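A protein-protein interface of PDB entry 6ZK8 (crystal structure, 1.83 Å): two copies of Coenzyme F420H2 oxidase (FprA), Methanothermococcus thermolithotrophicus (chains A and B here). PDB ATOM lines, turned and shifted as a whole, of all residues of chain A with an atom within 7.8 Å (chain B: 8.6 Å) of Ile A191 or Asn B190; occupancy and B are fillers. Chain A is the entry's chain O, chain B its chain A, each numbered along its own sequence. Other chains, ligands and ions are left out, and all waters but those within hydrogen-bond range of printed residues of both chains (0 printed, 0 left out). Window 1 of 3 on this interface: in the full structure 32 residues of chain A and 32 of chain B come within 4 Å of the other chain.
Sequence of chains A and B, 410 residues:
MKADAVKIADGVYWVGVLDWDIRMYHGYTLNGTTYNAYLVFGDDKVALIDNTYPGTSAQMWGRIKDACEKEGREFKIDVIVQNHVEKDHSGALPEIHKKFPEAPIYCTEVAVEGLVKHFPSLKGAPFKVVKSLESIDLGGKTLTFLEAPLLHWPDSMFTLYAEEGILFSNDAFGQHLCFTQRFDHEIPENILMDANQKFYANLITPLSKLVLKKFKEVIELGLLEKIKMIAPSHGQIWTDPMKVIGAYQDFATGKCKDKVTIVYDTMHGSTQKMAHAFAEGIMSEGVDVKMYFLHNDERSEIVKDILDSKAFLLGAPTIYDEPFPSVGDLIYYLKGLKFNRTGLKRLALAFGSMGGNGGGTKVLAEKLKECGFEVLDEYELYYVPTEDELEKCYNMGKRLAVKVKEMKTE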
ATOM      1  N   GLN A 175      -2.264 -14.014  -5.502  1.00  0.00           N
ATOM      2  CA  GLN A 175      -3.232 -14.259  -4.440  1.00  0.00           C
ATOM      3  C   GLN A 175      -3.603 -12.924  -3.801  1.00  0.00           C
ATOM      4  O   GLN A 175      -2.791 -11.987  -3.755  1.00  0.00           O
ATOM      5  CB  GLN A 175      -2.712 -15.227  -3.375  1.00  0.00           C
ATOM      6  CG  GLN A 175      -1.449 -15.965  -3.765  1.00  0.00           C
ATOM      7  CD  GLN A 175      -0.199 -15.123  -3.588  1.00  0.00           C
ATOM      8  OE1 GLN A 175      -0.016 -14.513  -2.554  1.00  0.00           O
ATOM      9  NE2 GLN A 175       0.669 -15.098  -4.598  1.00  0.00           N
ATOM     10  N   HIS A 176      -4.852 -12.827  -3.343  1.00  0.00           N
ATOM     11  CA  HIS A 176      -5.345 -11.588  -2.747  1.00  0.00           C
ATOM     12  C   HIS A 176      -5.030 -11.607  -1.260  1.00  0.00           C
ATOM     13  O   HIS A 176      -5.784 -12.122  -0.429  1.00  0.00           O
ATOM     14  CB  HIS A 176      -6.823 -11.405  -3.039  1.00  0.00           C
ATOM     15  CG  HIS A 176      -7.097 -10.961  -4.435  1.00  0.00           C
ATOM     16  ND1 HIS A 176      -6.448  -9.895  -5.015  1.00  0.00           N
ATOM     17  CD2 HIS A 176      -7.959 -11.430  -5.365  1.00  0.00           C
ATOM     18  CE1 HIS A 176      -6.887  -9.734  -6.251  1.00  0.00           C
ATOM     19  NE2 HIS A 176      -7.807 -10.652  -6.488  1.00  0.00           N
ATOM     20  N   LEU A 177      -3.861 -11.080  -0.943  1.00  0.00           N
ATOM     21  CA  LEU A 177      -3.356 -10.971   0.405  1.00  0.00           C
ATOM     22  C   LEU A 177      -2.663  -9.628   0.517  1.00  0.00           C
ATOM     23  O   LEU A 177      -1.981  -9.218  -0.420  1.00  0.00           O
ATOM     24  CB  LEU A 177      -2.374 -12.087   0.707  1.00  0.00           C
ATOM     25  CG  LEU A 177      -2.911 -13.506   0.729  1.00  0.00           C
ATOM     26  CD1 LEU A 177      -1.749 -14.506   0.819  1.00  0.00           C
ATOM     27  CD2 LEU A 177      -3.859 -13.676   1.892  1.00  0.00           C
ATOM     28  N   PHE A 179      -0.131  -8.099   3.154  1.00  0.00           N
ATOM     29  CA  PHE A 179       0.748  -8.176   4.307  1.00  0.00           C
ATOM     30  C   PHE A 179       1.928  -7.234   4.122  1.00  0.00           C
ATOM     31  O   PHE A 179       2.260  -6.829   3.004  1.00  0.00           O
ATOM     32  CB  PHE A 179       1.290  -9.596   4.534  1.00  0.00           C
ATOM     33  CG  PHE A 179       0.248 -10.599   4.876  1.00  0.00           C
ATOM     34  CD1 PHE A 179      -0.459 -10.496   6.057  1.00  0.00           C
ATOM     35  CD2 PHE A 179      -0.039 -11.658   4.023  1.00  0.00           C
ATOM     36  CE1 PHE A 179      -1.432 -11.440   6.389  1.00  0.00           C
ATOM     37  CE2 PHE A 179      -1.010 -12.578   4.338  1.00  0.00           C
ATOM     38  CZ  PHE A 179      -1.704 -12.477   5.519  1.00  0.00           C
ATOM     39  N   ILE A 187       4.961 -15.842   5.408  1.00  0.00           N
ATOM     40  CA  ILE A 187       3.619 -15.940   5.998  1.00  0.00           C
ATOM     41  C   ILE A 187       3.295 -17.390   6.165  1.00  0.00           C
ATOM     42  O   ILE A 187       3.966 -18.279   5.590  1.00  0.00           O
ATOM     43  CB  ILE A 187       2.566 -15.198   5.128  1.00  0.00           C
ATOM     44  CG1 ILE A 187       2.388 -15.868   3.783  1.00  0.00           C
ATOM     45  CG2 ILE A 187       2.941 -13.746   4.929  1.00  0.00           C
ATOM     46  CD1 ILE A 187       1.161 -15.418   3.056  1.00  0.00           C
ATOM     47  N   PRO A 188       2.272 -17.729   6.972  1.00  0.00           N
ATOM     48  CA  PRO A 188       1.883 -19.131   7.172  1.00  0.00           C
ATOM     49  C   PRO A 188       1.452 -19.775   5.867  1.00  0.00           C
ATOM     50  O   PRO A 188       0.747 -19.173   5.057  1.00  0.00           O
ATOM     51  CB  PRO A 188       0.712 -19.055   8.162  1.00  0.00           C
ATOM     52  CG  PRO A 188       0.865 -17.731   8.865  1.00  0.00           C
ATOM     53  CD  PRO A 188       1.469 -16.802   7.805  1.00  0.00           C
ATOM     54  N   GLU A 189       1.888 -21.013   5.672  1.00  0.00           N
ATOM     55  CA  GLU A 189       1.619 -21.710   4.421  1.00  0.00           C
ATOM     56  C   GLU A 189       0.132 -21.848   4.176  1.00  0.00           C
ATOM     57  O   GLU A 189      -0.334 -21.686   3.041  1.00  0.00           O
ATOM     58  CB  GLU A 189       2.251 -23.105   4.433  1.00  0.00           C
ATOM     59  CG  GLU A 189       2.524 -23.643   3.042  1.00  0.00           C
ATOM     60  CD  GLU A 189       2.339 -25.146   2.938  1.00  0.00           C
ATOM     61  OE1 GLU A 189       1.294 -25.641   3.440  1.00  0.00           O
ATOM     62  OE2 GLU A 189       3.204 -25.812   2.336  1.00  0.00           O
ATOM     63  N   ASN A 190      -0.630 -22.162   5.232  1.00  0.00           N
ATOM     64  CA  ASN A 190      -2.067 -22.364   5.090  1.00  0.00           C
ATOM     65  C   ASN A 190      -2.740 -21.125   4.521  1.00  0.00           C
ATOM     66  O   ASN A 190      -3.623 -21.219   3.668  1.00  0.00           O
ATOM     67  CB  ASN A 190      -2.672 -22.718   6.444  1.00  0.00           C
ATOM     68  CG  ASN A 190      -4.149 -22.486   6.485  1.00  0.00           C
ATOM     69  OD1 ASN A 190      -4.631 -21.513   7.083  1.00  0.00           O
ATOM     70  ND2 ASN A 190      -4.891 -23.366   5.847  1.00  0.00           N
ATOM     71  N   ILE A 191      -2.346 -19.948   4.993  1.00  0.00           N
ATOM     72  CA  ILE A 191      -2.915 -18.713   4.459  1.00  0.00           C
ATOM     73  C   ILE A 191      -2.527 -18.536   2.994  1.00  0.00           C
ATOM     74  O   ILE A 191      -3.372 -18.247   2.136  1.00  0.00           O
ATOM     75  CB  ILE A 191      -2.461 -17.520   5.315  1.00  0.00           C
ATOM     76  CG1 ILE A 191      -3.048 -17.647   6.721  1.00  0.00           C
ATOM     77  CG2 ILE A 191      -2.908 -16.212   4.679  1.00  0.00           C
ATOM     78  CD1 ILE A 191      -2.474 -16.668   7.726  1.00  0.00           C
ATOM     79  N   LEU A 192      -1.247 -18.732   2.689  1.00  0.00           N
ATOM     80  CA  LEU A 192      -0.763 -18.596   1.319  1.00  0.00           C
ATOM     81  C   LEU A 192      -1.525 -19.509   0.361  1.00  0.00           C
ATOM     82  O   LEU A 192      -2.041 -19.066  -0.668  1.00  0.00           O
ATOM     83  CB  LEU A 192       0.728 -18.927   1.271  1.00  0.00           C
ATOM     84  CG  LEU A 192       1.391 -18.968  -0.104  1.00  0.00           C
ATOM     85  CD1 LEU A 192       1.363 -17.619  -0.748  1.00  0.00           C
ATOM     86  CD2 LEU A 192       2.815 -19.490   0.006  1.00  0.00           C
ATOM     87  N   MET A 193      -1.600 -20.798   0.678  1.00  0.00           N
ATOM     88  CA  MET A 193      -2.179 -21.734  -0.272  1.00  0.00           C
ATOM     89  C   MET A 193      -3.694 -21.656  -0.307  1.00  0.00           C
ATOM     90  O   MET A 193      -4.284 -21.891  -1.366  1.00  0.00           O
ATOM     91  CB  MET A 193      -1.723 -23.149   0.059  1.00  0.00           C
ATOM     92  CG  MET A 193      -0.179 -23.320   0.055  1.00  0.00           C
ATOM     93  SD  MET A 193       0.636 -22.631  -1.425  1.00  0.00           S
ATOM     94  CE  MET A 193       0.126 -23.816  -2.670  1.00  0.00           C
ATOM     95  N   ASP A 194      -4.342 -21.312   0.809  1.00  0.00           N
ATOM     96  CA  ASP A 194      -5.792 -21.122   0.773  1.00  0.00           C
ATOM     97  C   ASP A 194      -6.131 -19.955  -0.133  1.00  0.00           C
ATOM     98  O   ASP A 194      -7.083 -20.022  -0.921  1.00  0.00           O
ATOM     99  CB  ASP A 194      -6.336 -20.904   2.200  1.00  0.00           C
ATOM    100  CG  ASP A 194      -7.854 -20.823   2.269  1.00  0.00           C
ATOM    101  OD1 ASP A 194      -8.571 -21.802   1.984  1.00  0.00           O
ATOM    102  OD2 ASP A 194      -8.379 -19.753   2.635  1.00  0.00           O
ATOM    103  N   ALA A 195      -5.328 -18.895  -0.072  1.00  0.00           N
ATOM    104  CA  ALA A 195      -5.553 -17.741  -0.939  1.00  0.00           C
ATOM    105  C   ALA A 195      -5.236 -18.076  -2.382  1.00  0.00           C
ATOM    106  O   ALA A 195      -5.949 -17.647  -3.295  1.00  0.00           O
ATOM    107  CB  ALA A 195      -4.722 -16.553  -0.465  1.00  0.00           C
ATOM    108  N   ASN A 196      -4.177 -18.863  -2.609  1.00  0.00           N
ATOM    109  CA  ASN A 196      -3.918 -19.336  -3.959  1.00  0.00           C
ATOM    110  C   ASN A 196      -5.088 -20.164  -4.484  1.00  0.00           C
ATOM    111  O   ASN A 196      -5.451 -20.056  -5.655  1.00  0.00           O
ATOM    112  CB  ASN A 196      -2.631 -20.141  -4.001  1.00  0.00           C
ATOM    113  CG  ASN A 196      -2.296 -20.608  -5.391  1.00  0.00           C
ATOM    114  OD1 ASN A 196      -2.015 -19.814  -6.285  1.00  0.00           O
ATOM    115  ND2 ASN A 196      -2.292 -21.912  -5.577  1.00  0.00           N
ATOM    116  N   GLN A 197      -5.665 -21.020  -3.640  1.00  0.00           N
ATOM    117  CA  GLN A 197      -6.803 -21.832  -4.059  1.00  0.00           C
ATOM    118  C   GLN A 197      -8.006 -20.962  -4.386  1.00  0.00           C
ATOM    119  O   GLN A 197      -8.722 -21.210  -5.367  1.00  0.00           O
ATOM    120  CB  GLN A 197      -7.139 -22.832  -2.961  1.00  0.00           C
ATOM    121  CG  GLN A 197      -8.269 -23.802  -3.321  1.00  0.00           C
ATOM    122  CD  GLN A 197      -8.475 -24.877  -2.270  1.00  0.00           C
ATOM    123  OE1 GLN A 197      -7.519 -25.381  -1.683  1.00  0.00           O
ATOM    124  NE2 GLN A 197      -9.739 -25.248  -2.040  1.00  0.00           N
ATOM    125  N   LYS A 198      -8.263 -19.944  -3.562  1.00  0.00           N
ATOM    126  CA  LYS A 198      -9.388 -19.055  -3.839  1.00  0.00           C
ATOM    127  C   LYS A 198      -9.174 -18.299  -5.141  1.00  0.00           C
ATOM    128  O   LYS A 198     -10.098 -18.149  -5.940  1.00  0.00           O
ATOM    129  CB  LYS A 198      -9.596 -18.085  -2.684  1.00  0.00           C
ATOM    130  CG  LYS A 198     -10.886 -17.305  -2.783  1.00  0.00           C
ATOM    131  CD  LYS A 198     -11.118 -16.434  -1.566  1.00  0.00           C
ATOM    132  CE  LYS A 198     -12.436 -15.739  -1.608  1.00  0.00           C
ATOM    133  NZ  LYS A 198     -12.672 -14.956  -0.381  1.00  0.00           N
ATOM    134  N   GLN A 236       1.833 -12.452  -2.609  1.00  0.00           N
ATOM    135  CA  GLN A 236       3.195 -12.811  -2.278  1.00  0.00           C
ATOM    136  C   GLN A 236       3.990 -13.195  -3.512  1.00  0.00           C
ATOM    137  O   GLN A 236       3.463 -13.751  -4.481  1.00  0.00           O
ATOM    138  CB  GLN A 236       3.220 -13.984  -1.292  1.00  0.00           C
ATOM    139  CG  GLN A 236       2.319 -13.819  -0.095  1.00  0.00           C
ATOM    140  CD  GLN A 236       2.535 -12.523   0.603  1.00  0.00           C
ATOM    141  OE1 GLN A 236       1.696 -11.620   0.551  1.00  0.00           O
ATOM    142  NE2 GLN A 236       3.664 -12.399   1.235  1.00  0.00           N
ATOM    143  N   LEU B 177     -14.532 -22.571  16.110  1.00  0.00           N
ATOM    144  CA  LEU B 177     -14.231 -23.248  14.863  1.00  0.00           C
ATOM    145  C   LEU B 177     -15.254 -24.349  14.690  1.00  0.00           C
ATOM    146  O   LEU B 177     -15.587 -25.028  15.664  1.00  0.00           O
ATOM    147  CB  LEU B 177     -12.827 -23.826  14.884  1.00  0.00           C
ATOM    148  CG  LEU B 177     -11.659 -22.839  14.923  1.00  0.00           C
ATOM    149  CD1 LEU B 177     -10.344 -23.560  15.214  1.00  0.00           C
ATOM    150  CD2 LEU B 177     -11.541 -22.074  13.638  1.00  0.00           C
ATOM    151  N   ASP B 184      -7.116 -30.969  17.903  1.00  0.00           N
ATOM    152  CA  ASP B 184      -6.210 -29.887  17.532  1.00  0.00           C
ATOM    153  C   ASP B 184      -5.265 -30.287  16.395  1.00  0.00           C
ATOM    154  O   ASP B 184      -5.038 -29.511  15.465  1.00  0.00           O
ATOM    155  CB  ASP B 184      -5.417 -29.418  18.757  1.00  0.00           C
ATOM    156  CG  ASP B 184      -4.761 -30.549  19.527  1.00  0.00           C
ATOM    157  OD1 ASP B 184      -5.013 -31.765  19.285  1.00  0.00           O
ATOM    158  OD2 ASP B 184      -3.951 -30.227  20.421  1.00  0.00           O
ATOM    159  N   ILE B 187      -6.255 -30.126  12.237  1.00  0.00           N
ATOM    160  CA  ILE B 187      -6.444 -28.935  11.397  1.00  0.00           C
ATOM    161  C   ILE B 187      -5.146 -28.162  11.376  1.00  0.00           C
ATOM    162  O   ILE B 187      -4.274 -28.364  12.232  1.00  0.00           O
ATOM    163  CB  ILE B 187      -7.599 -28.041  11.910  1.00  0.00           C
ATOM    164  CG1 ILE B 187      -7.273 -27.468  13.292  1.00  0.00           C
ATOM    165  CG2 ILE B 187      -8.940 -28.807  11.988  1.00  0.00           C
ATOM    166  CD1 ILE B 187      -8.238 -26.340  13.698  1.00  0.00           C
ATOM    167  N   PRO B 188      -4.977 -27.240  10.431  1.00  0.00           N
ATOM    168  CA  PRO B 188      -3.734 -26.460  10.369  1.00  0.00           C
ATOM    169  C   PRO B 188      -3.511 -25.668  11.647  1.00  0.00           C
ATOM    170  O   PRO B 188      -4.423 -25.025  12.173  1.00  0.00           O
ATOM    171  CB  PRO B 188      -3.946 -25.527   9.164  1.00  0.00           C
ATOM    172  CG  PRO B 188      -4.993 -26.210   8.326  1.00  0.00           C
ATOM    173  CD  PRO B 188      -5.911 -26.913   9.337  1.00  0.00           C
ATOM    174  N   GLU B 189      -2.263 -25.676  12.103  1.00  0.00           N
ATOM    175  CA  GLU B 189      -1.923 -25.020  13.358  1.00  0.00           C
ATOM    176  C   GLU B 189      -2.269 -23.546  13.331  1.00  0.00           C
ATOM    177  O   GLU B 189      -2.708 -23.004  14.342  1.00  0.00           O
ATOM    178  CB  GLU B 189      -0.439 -25.217  13.670  1.00  0.00           C
ATOM    179  CG  GLU B 189      -0.105 -25.115  15.153  1.00  0.00           C
ATOM    180  CD  GLU B 189       1.297 -24.632  15.424  1.00  0.00           C
ATOM    181  OE1 GLU B 189       2.254 -25.233  14.883  1.00  0.00           O
ATOM    182  OE2 GLU B 189       1.453 -23.660  16.195  1.00  0.00           O
ATOM    183  N   ASN B 190      -2.040 -22.873  12.200  1.00  0.00           N
ATOM    184  CA  ASN B 190      -2.304 -21.441  12.112  1.00  0.00           C
ATOM    185  C   ASN B 190      -3.766 -21.122  12.374  1.00  0.00           C
ATOM    186  O   ASN B 190      -4.092 -20.146  13.061  1.00  0.00           O
ATOM    187  CB  ASN B 190      -1.903 -20.937  10.732  1.00  0.00           C
ATOM    188  CG  ASN B 190      -2.553 -19.619  10.388  1.00  0.00           C
ATOM    189  OD1 ASN B 190      -3.471 -19.548   9.564  1.00  0.00           O
ATOM    190  ND2 ASN B 190      -2.108 -18.565  11.049  1.00  0.00           N
ATOM    191  N   ILE B 191      -4.661 -21.916  11.802  1.00  0.00           N
ATOM    192  CA  ILE B 191      -6.080 -21.715  12.032  1.00  0.00           C
ATOM    193  C   ILE B 191      -6.409 -21.935  13.501  1.00  0.00           C
ATOM    194  O   ILE B 191      -7.118 -21.134  14.121  1.00  0.00           O
ATOM    195  CB  ILE B 191      -6.894 -22.641  11.112  1.00  0.00           C
ATOM    196  CG1 ILE B 191      -6.726 -22.199   9.663  1.00  0.00           C
ATOM    197  CG2 ILE B 191      -8.375 -22.628  11.498  1.00  0.00           C
ATOM    198  CD1 ILE B 191      -7.294 -23.187   8.647  1.00  0.00           C
ATOM    199  N   LEU B 192      -5.892 -23.019  14.078  1.00  0.00           N
ATOM    200  CA  LEU B 192      -6.154 -23.331  15.478  1.00  0.00           C
ATOM    201  C   LEU B 192      -5.716 -22.201  16.390  1.00  0.00           C
ATOM    202  O   LEU B 192      -6.491 -21.729  17.226  1.00  0.00           O
ATOM    203  CB  LEU B 192      -5.450 -24.614  15.864  1.00  0.00           C
ATOM    204  CG  LEU B 192      -5.482 -25.035  17.335  1.00  0.00           C
ATOM    205  CD1 LEU B 192      -6.907 -25.349  17.753  1.00  0.00           C
ATOM    206  CD2 LEU B 192      -4.555 -26.232  17.559  1.00  0.00           C
ATOM    207  N   MET B 193      -4.479 -21.745  16.236  1.00  0.00           N
ATOM    208  CA  MET B 193      -3.932 -20.772  17.169  1.00  0.00           C
ATOM    209  C   MET B 193      -4.459 -19.370  16.889  1.00  0.00           C
ATOM    210  O   MET B 193      -4.575 -18.573  17.819  1.00  0.00           O
ATOM    211  CB  MET B 193      -2.400 -20.813  17.125  1.00  0.00           C
ATOM    212  CG  MET B 193      -1.802 -22.159  17.428  1.00  0.00           C
ATOM    213  SD  MET B 193      -2.463 -22.928  18.959  1.00  0.00           S
ATOM    214  CE  MET B 193      -1.663 -21.956  20.222  1.00  0.00           C
ATOM    215  N   ASP B 194      -4.789 -19.040  15.638  1.00  0.00           N
ATOM    216  CA  ASP B 194      -5.409 -17.742  15.381  1.00  0.00           C
ATOM    217  C   ASP B 194      -6.794 -17.687  16.022  1.00  0.00           C
ATOM    218  O   ASP B 194      -7.181 -16.669  16.595  1.00  0.00           O
ATOM    219  CB  ASP B 194      -5.453 -17.457  13.867  1.00  0.00           C
ATOM    220  CG  ASP B 194      -6.012 -16.071  13.554  1.00  0.00           C
ATOM    221  OD1 ASP B 194      -5.401 -15.057  13.932  1.00  0.00           O
ATOM    222  OD2 ASP B 194      -7.099 -15.974  12.968  1.00  0.00           O
ATOM    223  N   ALA B 195      -7.542 -18.791  15.969  1.00  0.00           N
ATOM    224  CA  ALA B 195      -8.845 -18.859  16.631  1.00  0.00           C
ATOM    225  C   ALA B 195      -8.706 -18.838  18.150  1.00  0.00           C
ATOM    226  O   ALA B 195      -9.481 -18.179  18.854  1.00  0.00           O
ATOM    227  CB  ALA B 195      -9.568 -20.124  16.197  1.00  0.00           C
ATOM    228  N   ASN B 196      -7.719 -19.540  18.678  1.00  0.00           N
ATOM    229  CA  ASN B 196      -7.444 -19.425  20.103  1.00  0.00           C
ATOM    230  C   ASN B 196      -7.109 -17.982  20.497  1.00  0.00           C
ATOM    231  O   ASN B 196      -7.545 -17.499  21.549  1.00  0.00           O
ATOM    232  CB  ASN B 196      -6.300 -20.364  20.471  1.00  0.00           C
ATOM    233  CG  ASN B 196      -6.019 -20.370  21.934  1.00  0.00           C
ATOM    234  OD1 ASN B 196      -6.870 -20.792  22.731  1.00  0.00           O
ATOM    235  ND2 ASN B 196      -4.837 -19.926  22.313  1.00  0.00           N
ATOM    236  N   GLN B 197      -6.323 -17.281  19.678  1.00  0.00           N
ATOM    237  CA  GLN B 197      -5.966 -15.902  20.000  1.00  0.00           C
ATOM    238  C   GLN B 197      -7.198 -15.004  19.990  1.00  0.00           C
ATOM    239  O   GLN B 197      -7.379 -14.182  20.893  1.00  0.00           O
ATOM    240  CB  GLN B 197      -4.908 -15.388  19.020  1.00  0.00           C
ATOM    241  CG  GLN B 197      -4.401 -13.986  19.317  1.00  0.00           C
ATOM    242  CD  GLN B 197      -3.241 -13.573  18.418  1.00  0.00           C
ATOM    243  OE1 GLN B 197      -2.384 -14.373  18.098  1.00  0.00           O
ATOM    244  NE2 GLN B 197      -3.225 -12.319  18.000  1.00  0.00           N
ATOM    245  N   LYS B 243       0.257 -26.796  24.805  1.00  0.00           N
ATOM    246  CA  LYS B 243       0.290 -25.797  23.740  1.00  0.00           C
ATOM    247  C   LYS B 243      -0.656 -24.638  24.038  1.00  0.00           C
ATOM    248  O   LYS B 243      -0.298 -23.469  23.864  1.00  0.00           O
ATOM    249  CB  LYS B 243      -0.072 -26.443  22.406  1.00  0.00           C
ATOM    250  CG  LYS B 243       0.083 -25.513  21.228  1.00  0.00           C
ATOM    251  CD  LYS B 243       0.178 -26.285  19.911  1.00  0.00           C
ATOM    252  CE  LYS B 243       0.385 -25.332  18.718  1.00  0.00           C
ATOM    253  NZ  LYS B 243       1.780 -24.767  18.656  1.00  0.00           N
ATOM    254  N   LYS B 257       4.488  -9.184  19.775  1.00  0.00           N
ATOM    255  CA  LYS B 257       5.400  -9.111  18.645  1.00  0.00           C
ATOM    256  C   LYS B 257       5.741  -7.657  18.315  1.00  0.00           C
ATOM    257  O   LYS B 257       5.123  -6.712  18.813  1.00  0.00           O
ATOM    258  CB  LYS B 257       4.775  -9.793  17.430  1.00  0.00           C
ATOM    259  CG  LYS B 257       4.416 -11.245  17.648  1.00  0.00           C
ATOM    260  CD  LYS B 257       3.696 -11.803  16.433  1.00  0.00           C
ATOM    261  CE  LYS B 257       3.500 -13.322  16.547  1.00  0.00           C
ATOM    262  NZ  LYS B 257       2.845 -13.869  15.278  1.00  0.00           N
ATOM    263  N   LYS B 290      -0.973  -4.138  11.052  1.00  0.00           N
ATOM    264  CA  LYS B 290      -2.327  -4.550  10.708  1.00  0.00           C
ATOM    265  C   LYS B 290      -3.172  -3.292  10.581  1.00  0.00           C
ATOM    266  O   LYS B 290      -3.124  -2.416  11.445  1.00  0.00           O
ATOM    267  CB  LYS B 290      -2.906  -5.490  11.762  1.00  0.00           C
ATOM    268  CG  LYS B 290      -2.060  -6.737  12.002  1.00  0.00           C
ATOM    269  CD  LYS B 290      -2.077  -7.701  10.799  1.00  0.00           C
ATOM    270  CE  LYS B 290      -1.058  -8.820  11.014  1.00  0.00           C
ATOM    271  NZ  LYS B 290      -1.043  -9.830   9.917  1.00  0.00           N
ATOM    272  N   LYS B 304      -8.226  -8.952  18.486  1.00  0.00           N
ATOM    273  CA  LYS B 304      -7.366 -10.105  18.268  1.00  0.00           C
ATOM    274  C   LYS B 304      -5.932  -9.668  17.970  1.00  0.00           C
ATOM    275  O   LYS B 304      -4.968 -10.160  18.575  1.00  0.00           O
ATOM    276  CB  LYS B 304      -7.923 -10.939  17.114  1.00  0.00           C
ATOM    277  CG  LYS B 304      -7.076 -12.179  16.827  1.00  0.00           C
ATOM    278  CD  LYS B 304      -7.457 -12.809  15.482  1.00  0.00           C
ATOM    279  CE  LYS B 304      -6.750 -12.113  14.337  1.00  0.00           C
ATOM    280  NZ  LYS B 304      -7.038 -12.802  13.037  1.00  0.00           N
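The side-chain amide oxygen (OD1) of Asn B190 lies close to the side-chain amide oxygen (OD1) of Asn A190 (3.4 Å).
CE1 of Phe A179 touches NZ of Lys B290, 3.9 Å away.
CG of Pro A188 touches ND2 of Asn B190, at 3.8 Å.
Pro B188 touches Asn A190.
OD1 of Asn A190 touches CG1 of Ile B191, 3.4 Å away.
Ile A191 touches Asn B190 (CG1 to OD1, 3.4 Å).
Of the printed residues of chain B, Pro A188 touches Asn B190 (3.8 Å).
Of chain B, only Pro B188, Asn B190 and Ile B191 come within 4 Å of Asn A190.
Of chain B, only Asn B190 (3.4 Å) comes within 4 Å of Ile A191.
Asn B190 touches just these residues of chain A: Pro A188 (3.8 Å), Asn A190 (3.4 Å) and Ile A191 (3.4 Å).
Of the printed residues of chain A, Ile B191 touches Asn A190 (3.4 Å).
Met B193 touches none of the printed residues of chain A.
Asp B194 touches none of the printed residues of chain A.
The nearest printed residue of chain B that does not touch Pro A188 is Ile B191 (7.1 Å).
Of the 17 printed residues of chain B, 4 touch a printed residue of chain A.
Of the 17 printed residues of chain A, 4 touch a printed residue of chain B.
Printed residues of chain A that touch a printed residue of chain B: Phe A179, Pro A188, Asn A190 and Ile A191.
Hydrophobic or aromatic side chains of chain A that line the printed part of chain B: Phe A179, Pro A188 and Ile A191.
Among the printed residues, 6 pairs touch across the chains.
Among the printed residues, no Asp or Glu carboxylate lies within 4 Å of a Lys or Arg side-chain nitrogen of the other chain.
Pro A188 touches Asn B190, and with the chains exchanged Asn A190 touches Pro B188.
Asn A190 touches its own counterpart, Asn B190.
Asn A190 touches Ile B191, and with the chains exchanged Ile A191 touches Asn B190.
Positions printed for both chains: 177, 187, 188, 189, 190, 191, 192, 193, 194, 195, 196 and 197.
Of the 6 pairs that touch across the chains among the printed residues, 5 have their exchanged pair printed and touching as well.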
